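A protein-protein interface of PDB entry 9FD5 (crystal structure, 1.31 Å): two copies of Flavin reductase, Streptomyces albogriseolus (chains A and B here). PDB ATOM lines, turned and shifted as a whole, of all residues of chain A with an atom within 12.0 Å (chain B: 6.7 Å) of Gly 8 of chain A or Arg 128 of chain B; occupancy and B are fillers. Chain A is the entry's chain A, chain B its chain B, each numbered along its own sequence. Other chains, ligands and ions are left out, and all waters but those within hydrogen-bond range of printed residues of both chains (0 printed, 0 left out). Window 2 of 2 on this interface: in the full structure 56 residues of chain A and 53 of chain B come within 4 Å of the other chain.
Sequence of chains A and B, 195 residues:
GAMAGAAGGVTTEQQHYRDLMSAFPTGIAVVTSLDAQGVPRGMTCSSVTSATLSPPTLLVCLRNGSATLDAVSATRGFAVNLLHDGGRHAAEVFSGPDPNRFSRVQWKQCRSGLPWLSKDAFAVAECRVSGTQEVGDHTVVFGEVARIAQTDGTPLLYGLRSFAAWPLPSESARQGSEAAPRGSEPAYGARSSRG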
ATOM      1  N   GLY A   8     -36.538 -23.984   2.664  1.00  0.00           N
ATOM      2  CA  GLY A   8     -35.881 -23.881   3.962  1.00  0.00           C
ATOM      3  C   GLY A   8     -36.526 -22.909   4.948  1.00  0.00           C
ATOM      4  O   GLY A   8     -36.437 -23.080   6.177  1.00  0.00           O
ATOM      5  N   GLY A   9     -37.145 -21.870   4.400  1.00  0.00           N
ATOM      6  CA  GLY A   9     -37.876 -20.879   5.179  1.00  0.00           C
ATOM      7  C   GLY A   9     -37.947 -19.583   4.381  1.00  0.00           C
ATOM      8  O   GLY A   9     -37.841 -19.597   3.169  1.00  0.00           O
ATOM      9  N   VAL A  10     -38.138 -18.466   5.081  1.00  0.00           N
ATOM     10  CA  VAL A  10     -38.206 -17.190   4.382  1.00  0.00           C
ATOM     11  C   VAL A  10     -36.876 -16.896   3.697  1.00  0.00           C
ATOM     12  O   VAL A  10     -35.796 -17.114   4.260  1.00  0.00           O
ATOM     13  CB  VAL A  10     -38.582 -16.073   5.366  1.00  0.00           C
ATOM     14  CG1 VAL A  10     -38.627 -14.703   4.667  1.00  0.00           C
ATOM     15  CG2 VAL A  10     -39.941 -16.370   6.008  1.00  0.00           C
ATOM     16  N   THR A  11     -36.955 -16.411   2.457  1.00  0.00           N
ATOM     17  CA  THR A  11     -35.784 -15.965   1.708  1.00  0.00           C
ATOM     18  C   THR A  11     -35.890 -14.469   1.453  1.00  0.00           C
ATOM     19  O   THR A  11     -36.974 -13.924   1.245  1.00  0.00           O
ATOM     20  CB  THR A  11     -35.665 -16.689   0.384  1.00  0.00           C
ATOM     21  OG1 THR A  11     -36.869 -16.514  -0.367  1.00  0.00           O
ATOM     22  CG2 THR A  11     -35.433 -18.188   0.612  1.00  0.00           C
ATOM     23  N   THR A  12     -34.758 -13.781   1.442  1.00  0.00           N
ATOM     24  CA  THR A  12     -34.823 -12.356   1.134  1.00  0.00           C
ATOM     25  C   THR A  12     -35.078 -12.126  -0.346  1.00  0.00           C
ATOM     26  O   THR A  12     -34.690 -12.924  -1.201  1.00  0.00           O
ATOM     27  CB  THR A  12     -33.518 -11.700   1.593  1.00  0.00           C
ATOM     28  OG1 THR A  12     -33.692 -10.285   1.626  1.00  0.00           O
ATOM     29  CG2 THR A  12     -32.322 -12.048   0.694  1.00  0.00           C
ATOM     30  N   GLU A  13     -35.738 -11.019  -0.646  1.00  0.00           N
ATOM     31  CA  GLU A  13     -35.941 -10.657  -2.035  1.00  0.00           C
ATOM     32  C   GLU A  13     -34.599 -10.460  -2.734  1.00  0.00           C
ATOM     33  O   GLU A  13     -33.638  -9.966  -2.147  1.00  0.00           O
ATOM     34  CB  GLU A  13     -36.755  -9.371  -2.119  1.00  0.00           C
ATOM     35  CG  GLU A  13     -38.258  -9.567  -1.869  1.00  0.00           C
ATOM     36  CD  GLU A  13     -38.971 -10.173  -3.067  1.00  0.00           C
ATOM     37  OE1 GLU A  13     -38.444 -10.048  -4.205  1.00  0.00           O
ATOM     38  OE2 GLU A  13     -40.066 -10.769  -2.867  1.00  0.00           O
ATOM     39  N   TYR A  17     -30.899  -8.700  -1.488  1.00  0.00           N
ATOM     40  CA  TYR A  17     -29.637  -9.427  -1.465  1.00  0.00           C
ATOM     41  C   TYR A  17     -28.569  -8.749  -2.316  1.00  0.00           C
ATOM     42  O   TYR A  17     -27.415  -8.619  -1.898  1.00  0.00           O
ATOM     43  CB  TYR A  17     -29.868 -10.858  -1.920  1.00  0.00           C
ATOM     44  CG  TYR A  17     -28.603 -11.676  -1.960  1.00  0.00           C
ATOM     45  CD1 TYR A  17     -28.056 -12.217  -0.805  1.00  0.00           C
ATOM     46  CD2 TYR A  17     -27.924 -11.871  -3.147  1.00  0.00           C
ATOM     47  CE1 TYR A  17     -26.908 -12.942  -0.833  1.00  0.00           C
ATOM     48  CE2 TYR A  17     -26.753 -12.622  -3.190  1.00  0.00           C
ATOM     49  CZ  TYR A  17     -26.247 -13.161  -2.020  1.00  0.00           C
ATOM     50  OH  TYR A  17     -25.092 -13.886  -2.017  1.00  0.00           O
ATOM     51  N   LEU A  20     -27.212  -5.788  -0.557  1.00  0.00           N
ATOM     52  CA  LEU A  20     -26.319  -6.177   0.519  1.00  0.00           C
ATOM     53  C   LEU A  20     -24.947  -6.533  -0.026  1.00  0.00           C
ATOM     54  O   LEU A  20     -23.918  -6.023   0.424  1.00  0.00           O
ATOM     55  CB  LEU A  20     -26.908  -7.404   1.236  1.00  0.00           C
ATOM     56  CG  LEU A  20     -25.989  -8.125   2.253  1.00  0.00           C
ATOM     57  CD1 LEU A  20     -25.860  -7.277   3.525  1.00  0.00           C
ATOM     58  CD2 LEU A  20     -26.445  -9.594   2.481  1.00  0.00           C
ATOM     59  N   VAL A 135     -24.566 -25.182  -6.088  1.00  0.00           N
ATOM     60  CA  VAL A 135     -25.362 -24.366  -5.193  1.00  0.00           C
ATOM     61  C   VAL A 135     -26.315 -23.523  -6.047  1.00  0.00           C
ATOM     62  O   VAL A 135     -25.891 -22.596  -6.741  1.00  0.00           O
ATOM     63  CB  VAL A 135     -24.473 -23.504  -4.273  1.00  0.00           C
ATOM     64  CG1 VAL A 135     -23.437 -22.675  -5.053  1.00  0.00           C
ATOM     65  CG2 VAL A 135     -25.298 -22.639  -3.361  1.00  0.00           C
ATOM     66  N   PRO B  55     -32.034 -19.881  -4.092  1.00  0.00           N
ATOM     67  CA  PRO B  55     -32.402 -18.593  -3.492  1.00  0.00           C
ATOM     68  C   PRO B  55     -31.154 -17.857  -3.095  1.00  0.00           C
ATOM     69  O   PRO B  55     -30.086 -18.416  -3.186  1.00  0.00           O
ATOM     70  CB  PRO B  55     -33.209 -19.007  -2.279  1.00  0.00           C
ATOM     71  CG  PRO B  55     -32.508 -20.236  -1.819  1.00  0.00           C
ATOM     72  CD  PRO B  55     -32.023 -20.942  -3.078  1.00  0.00           C
ATOM     73  N   THR B  57     -28.037 -16.847  -1.590  1.00  0.00           N
ATOM     74  CA  THR B  57     -27.161 -17.654  -0.758  1.00  0.00           C
ATOM     75  C   THR B  57     -25.751 -17.108  -0.862  1.00  0.00           C
ATOM     76  O   THR B  57     -25.202 -16.970  -1.960  1.00  0.00           O
ATOM     77  CB  THR B  57     -27.162 -19.123  -1.229  1.00  0.00           C
ATOM     78  OG1 THR B  57     -28.498 -19.618  -1.308  1.00  0.00           O
ATOM     79  CG2 THR B  57     -26.339 -20.013  -0.308  1.00  0.00           C
ATOM     80  N   ARG B  76     -27.667 -23.614  13.310  1.00  0.00           N
ATOM     81  CA  ARG B  76     -27.992 -23.596  11.886  1.00  0.00           C
ATOM     82  C   ARG B  76     -28.429 -22.217  11.425  1.00  0.00           C
ATOM     83  O   ARG B  76     -29.218 -22.080  10.495  1.00  0.00           O
ATOM     84  CB  ARG B  76     -28.978 -24.701  11.497  1.00  0.00           C
ATOM     85  CG  ARG B  76     -28.323 -26.103  11.504  1.00  0.00           C
ATOM     86  CD  ARG B  76     -28.631 -26.835  12.776  1.00  0.00           C
ATOM     87  NE  ARG B  76     -29.936 -27.480  12.740  1.00  0.00           N
ATOM     88  CZ  ARG B  76     -30.684 -27.707  13.811  1.00  0.00           C
ATOM     89  NH1 ARG B  76     -30.325 -27.282  15.014  1.00  0.00           N
ATOM     90  NH2 ARG B  76     -31.830 -28.359  13.670  1.00  0.00           N
ATOM     91  N   GLY B  77     -27.879 -21.190  12.060  1.00  0.00           N
ATOM     92  CA  GLY B  77     -28.151 -19.827  11.668  1.00  0.00           C
ATOM     93  C   GLY B  77     -26.964 -18.976  12.044  1.00  0.00           C
ATOM     94  O   GLY B  77     -26.173 -19.335  12.929  1.00  0.00           O
ATOM     95  N   PHE B  78     -26.822 -17.858  11.345  1.00  0.00           N
ATOM     96  CA  PHE B  78     -25.770 -16.919  11.679  1.00  0.00           C
ATOM     97  C   PHE B  78     -26.091 -15.563  11.099  1.00  0.00           C
ATOM     98  O   PHE B  78     -26.884 -15.444  10.173  1.00  0.00           O
ATOM     99  CB  PHE B  78     -24.415 -17.391  11.196  1.00  0.00           C
ATOM    100  CG  PHE B  78     -24.293 -17.596   9.687  1.00  0.00           C
ATOM    101  CD1 PHE B  78     -24.705 -18.790   9.081  1.00  0.00           C
ATOM    102  CD2 PHE B  78     -23.698 -16.618   8.888  1.00  0.00           C
ATOM    103  CE1 PHE B  78     -24.510 -18.991   7.711  1.00  0.00           C
ATOM    104  CE2 PHE B  78     -23.527 -16.825   7.523  1.00  0.00           C
ATOM    105  CZ  PHE B  78     -23.910 -18.023   6.954  1.00  0.00           C
ATOM    106  N   GLU B 126     -29.293 -11.899   8.250  1.00  0.00           N
ATOM    107  CA  GLU B 126     -29.586 -13.108   9.002  1.00  0.00           C
ATOM    108  C   GLU B 126     -29.701 -14.261   8.016  1.00  0.00           C
ATOM    109  O   GLU B 126     -30.470 -14.183   7.046  1.00  0.00           O
ATOM    110  CB  GLU B 126     -30.918 -12.933   9.723  1.00  0.00           C
ATOM    111  CG  GLU B 126     -30.833 -11.965  10.863  1.00  0.00           C
ATOM    112  CD  GLU B 126     -32.018 -12.112  11.795  1.00  0.00           C
ATOM    113  OE1 GLU B 126     -32.960 -12.860  11.478  1.00  0.00           O
ATOM    114  OE2 GLU B 126     -31.989 -11.503  12.861  1.00  0.00           O
ATOM    115  N   CYS B 127     -28.954 -15.318   8.274  1.00  0.00           N
ATOM    116  CA  CYS B 127     -28.791 -16.438   7.367  1.00  0.00           C
ATOM    117  C   CYS B 127     -29.177 -17.751   8.043  1.00  0.00           C
ATOM    118  O   CYS B 127     -28.939 -17.951   9.236  1.00  0.00           O
ATOM    119  CB  CYS B 127     -27.331 -16.549   6.900  1.00  0.00           C
ATOM    120  SG  CYS B 127     -26.734 -15.066   6.092  1.00  0.00           S
ATOM    121  N   ARG B 128     -29.753 -18.643   7.262  1.00  0.00           N
ATOM    122  CA  ARG B 128     -29.979 -20.016   7.668  1.00  0.00           C
ATOM    123  C   ARG B 128     -28.903 -20.857   7.007  1.00  0.00           C
ATOM    124  O   ARG B 128     -28.611 -20.682   5.828  1.00  0.00           O
ATOM    125  CB  ARG B 128     -31.321 -20.517   7.139  1.00  0.00           C
ATOM    126  CG  ARG B 128     -32.507 -20.228   7.931  1.00  0.00           C
ATOM    127  CD  ARG B 128     -33.644 -21.113   7.365  1.00  0.00           C
ATOM    128  NE  ARG B 128     -33.762 -20.967   5.912  1.00  0.00           N
ATOM    129  CZ  ARG B 128     -34.344 -19.914   5.352  1.00  0.00           C
ATOM    130  NH1 ARG B 128     -34.891 -18.972   6.091  1.00  0.00           N
ATOM    131  NH2 ARG B 128     -34.384 -19.817   4.023  1.00  0.00           N
ATOM    132  N   VAL B 129     -28.363 -21.818   7.739  1.00  0.00           N
ATOM    133  CA  VAL B 129     -27.388 -22.747   7.173  1.00  0.00           C
ATOM    134  C   VAL B 129     -28.119 -23.741   6.291  1.00  0.00           C
ATOM    135  O   VAL B 129     -28.906 -24.553   6.787  1.00  0.00           O
ATOM    136  CB  VAL B 129     -26.596 -23.466   8.262  1.00  0.00           C
ATOM    137  CG1 VAL B 129     -25.675 -24.492   7.643  1.00  0.00           C
ATOM    138  CG2 VAL B 129     -25.779 -22.496   9.052  1.00  0.00           C
ATOM    139  N   SER B 130     -27.848 -23.704   4.996  1.00  0.00           N
ATOM    140  CA  SER B 130     -28.430 -24.649   4.065  1.00  0.00           C
ATOM    141  C   SER B 130     -27.529 -25.825   3.750  1.00  0.00           C
ATOM    142  O   SER B 130     -28.005 -26.832   3.177  1.00  0.00           O
ATOM    143  CB  SER B 130     -28.840 -23.933   2.778  1.00  0.00           C
ATOM    144  OG  SER B 130     -27.769 -23.256   2.237  1.00  0.00           O
ATOM    145  N   GLY B 131     -26.267 -25.730   4.114  1.00  0.00           N
ATOM    146  CA  GLY B 131     -25.346 -26.820   3.934  1.00  0.00           C
ATOM    147  C   GLY B 131     -23.969 -26.448   4.430  1.00  0.00           C
ATOM    148  O   GLY B 131     -23.653 -25.274   4.617  1.00  0.00           O
ATOM    149  N   VAL B 141     -19.574 -22.842   4.738  1.00  0.00           N
ATOM    150  CA  VAL B 141     -20.940 -22.793   5.265  1.00  0.00           C
ATOM    151  C   VAL B 141     -21.774 -22.000   4.271  1.00  0.00           C
ATOM    152  O   VAL B 141     -21.440 -20.849   3.957  1.00  0.00           O
ATOM    153  CB  VAL B 141     -21.004 -22.113   6.643  1.00  0.00           C
ATOM    154  CG1 VAL B 141     -22.442 -22.103   7.162  1.00  0.00           C
ATOM    155  CG2 VAL B 141     -20.067 -22.767   7.635  1.00  0.00           C
ATOM    156  N   PHE B 142     -22.836 -22.607   3.769  1.00  0.00           N
ATOM    157  CA  PHE B 142     -23.767 -21.949   2.866  1.00  0.00           C
ATOM    158  C   PHE B 142     -24.877 -21.334   3.698  1.00  0.00           C
ATOM    159  O   PHE B 142     -25.509 -22.018   4.497  1.00  0.00           O
ATOM    160  CB  PHE B 142     -24.304 -22.936   1.834  1.00  0.00           C
ATOM    161  CG  PHE B 142     -23.246 -23.460   0.912  1.00  0.00           C
ATOM    162  CD1 PHE B 142     -22.873 -22.722  -0.178  1.00  0.00           C
ATOM    163  CD2 PHE B 142     -22.530 -24.608   1.194  1.00  0.00           C
ATOM    164  CE1 PHE B 142     -21.885 -23.175  -1.026  1.00  0.00           C
ATOM    165  CE2 PHE B 142     -21.536 -25.054   0.346  1.00  0.00           C
ATOM    166  CZ  PHE B 142     -21.221 -24.342  -0.755  1.00  0.00           C
ATOM    167  N   GLY B 143     -25.081 -20.035   3.521  1.00  0.00           N
ATOM    168  CA  GLY B 143     -26.081 -19.267   4.229  1.00  0.00           C
ATOM    169  C   GLY B 143     -27.142 -18.728   3.313  1.00  0.00           C
ATOM    170  O   GLY B 143     -26.869 -17.856   2.503  1.00  0.00           O
ATOM    171  N   GLU B 144     -28.343 -19.265   3.416  1.00  0.00           N
ATOM    172  CA  GLU B 144     -29.492 -18.719   2.707  1.00  0.00           C
ATOM    173  C   GLU B 144     -29.961 -17.503   3.484  1.00  0.00           C
ATOM    174  O   GLU B 144     -30.275 -17.609   4.678  1.00  0.00           O
ATOM    175  CB  GLU B 144     -30.629 -19.744   2.598  1.00  0.00           C
ATOM    176  CG  GLU B 144     -30.428 -20.688   1.460  1.00  0.00           C
ATOM    177  CD  GLU B 144     -31.541 -21.709   1.319  1.00  0.00           C
ATOM    178  OE1 GLU B 144     -32.602 -21.582   1.997  1.00  0.00           O
ATOM    179  OE2 GLU B 144     -31.348 -22.624   0.498  1.00  0.00           O
ATOM    180  N   VAL B 145     -29.967 -16.347   2.818  1.00  0.00           N
ATOM    181  CA  VAL B 145     -30.251 -15.113   3.515  1.00  0.00           C
ATOM    182  C   VAL B 145     -31.755 -14.982   3.669  1.00  0.00           C
ATOM    183  O   VAL B 145     -32.502 -15.002   2.680  1.00  0.00           O
ATOM    184  CB  VAL B 145     -29.646 -13.925   2.769  1.00  0.00           C
ATOM    185  CG1 VAL B 145     -29.962 -12.640   3.510  1.00  0.00           C
ATOM    186  CG2 VAL B 145     -28.123 -14.099   2.606  1.00  0.00           C
ATOM    187  N   ALA B 146     -32.198 -14.774   4.907  1.00  0.00           N
ATOM    188  CA  ALA B 146     -33.609 -14.677   5.251  1.00  0.00           C
ATOM    189  C   ALA B 146     -34.085 -13.241   5.398  1.00  0.00           C
ATOM    190  O   ALA B 146     -35.224 -12.927   5.009  1.00  0.00           O
ATOM    191  CB  ALA B 146     -33.869 -15.430   6.556  1.00  0.00           C
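The side-chain hydroxyl (OG1) of Thr 57 of chain B lies within hydrogen-bond range of the backbone carbonyl oxygen (O) of Pro 55 of chain B, 2.7 Å away. The backbone NH (N) of Ala 146 of chain B lies within hydrogen-bond range of the backbone carbonyl oxygen (O) of Glu 126 of chain B, 2.8 Å away. OE1 of Glu 144 of chain B is in salt-bridge range of NH2 of Arg 128 of chain B (3.2 Å).
Among the printed residues, pairs that only touch across the chains: Val 10 of chain A with Ala 146 of chain B (3.4 Å), Thr 11 of chain A with Val 145 of chain B (3.6 Å), Thr 12 of chain A with Ala 146 of chain B (3.7 Å), Thr 11 of chain A with Pro 55 of chain B (3.7 Å), Tyr 17 of chain A with Val 145 of chain B (3.8 Å), Thr 11 of chain A with Arg 128 of chain B (3.9 Å) and Thr 11 of chain A with Ala 146 of chain B (3.9 Å).
Of chain B, only Arg 128 (3.4 Å) comes within 4 Å of Gly 8 of chain A. Arg 128 of chain B touches just these residues of chain A: Gly 8, Gly 9, Val 10 and Thr 11. No residue of chain A comes within 4 Å of Gly 77 of chain B. No residue of chain A comes within 4 Å of Phe 78 of chain B. Cys 127 of chain B touches none of the printed residues of chain A. No residue of chain A comes within 4 Å of Val 129 of chain B. No residue of chain A comes within 4 Å of Ser 130 of chain B. No residue of chain A comes within 4 Å of Gly 131 of chain B. No residue of chain A comes within 4 Å of Glu 144 of chain B. Val 145 of chain B touches just these residues of chain A: Thr 11, Thr 12 and Tyr 17. Ala 146 of chain B touches just these residues of chain A: Val 10, Thr 11 and Thr 12. Of the printed residues of chain B, Gly 9 of chain A touches Arg 128 (3.5 Å). Of the printed residues of chain B, Thr 12 of chain A touches Val 145 (2.8 Å) and Ala 146 (3.7 Å). Of the printed residues of chain B, Thr 11 of chain A touches Pro 55 (3.7 Å), Arg 128 (3.9 Å), Val 145 (3.6 Å) and Ala 146 (3.9 Å). The nearest residue of chain B that does not touch Gly 8 of chain A is Glu 144 of chain B (4.5 Å). The nearest printed residue of chain B that does not touch Gly 9 of chain A is Glu 144 of chain B (5.1 Å).
The backbone carbonyl oxygen (O) of Thr 57 of chain B sits at hydrogen-bond distance from the side-chain hydroxyl (OH) of Tyr 17 of chain A (3.1 Å). The backbone carbonyl oxygen (O) of Val 145 of chain B is in hydrogen-bond range of the backbone NH (N) of Thr 12 of chain A. The backbone NH (N) of Gly 9 of chain A lies close to the guanidinium group (NH2) of Arg 128 of chain B, at 3.5 Å. NH1 of Arg 128 of chain B sits at hydrogen-bond distance from O of Val 10 of chain A (2.8 Å). The backbone carbonyl oxygen (O) of Gly 8 of chain A sits at hydrogen-bond distance from the guanidinium group (NE) of Arg 128 of chain B (3.4 Å).
Of the 9 printed residues of chain A, 6 touch a printed residue of chain B. Hydrophobic or aromatic side chains of chain A within 4 Å of the printed part of chain B: Val 10 and Tyr 17. Of the 17 printed residues of chain B, 5 touch a printed residue of chain A. Hydrophobic or aromatic side chains of chain B that line the printed part of chain A: Pro 55, Val 145 and Ala 146. Among the printed residues, 12 pairs touch across the chains. Among the printed residues, no Asp or Glu carboxylate lies within 4 Å of a Lys or Arg side-chain nitrogen of the other chain.
No position is printed for both chains. Of the 12 pairs that touch across the chains among the printed residues, none has its exchanged pair printed and touching as well.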
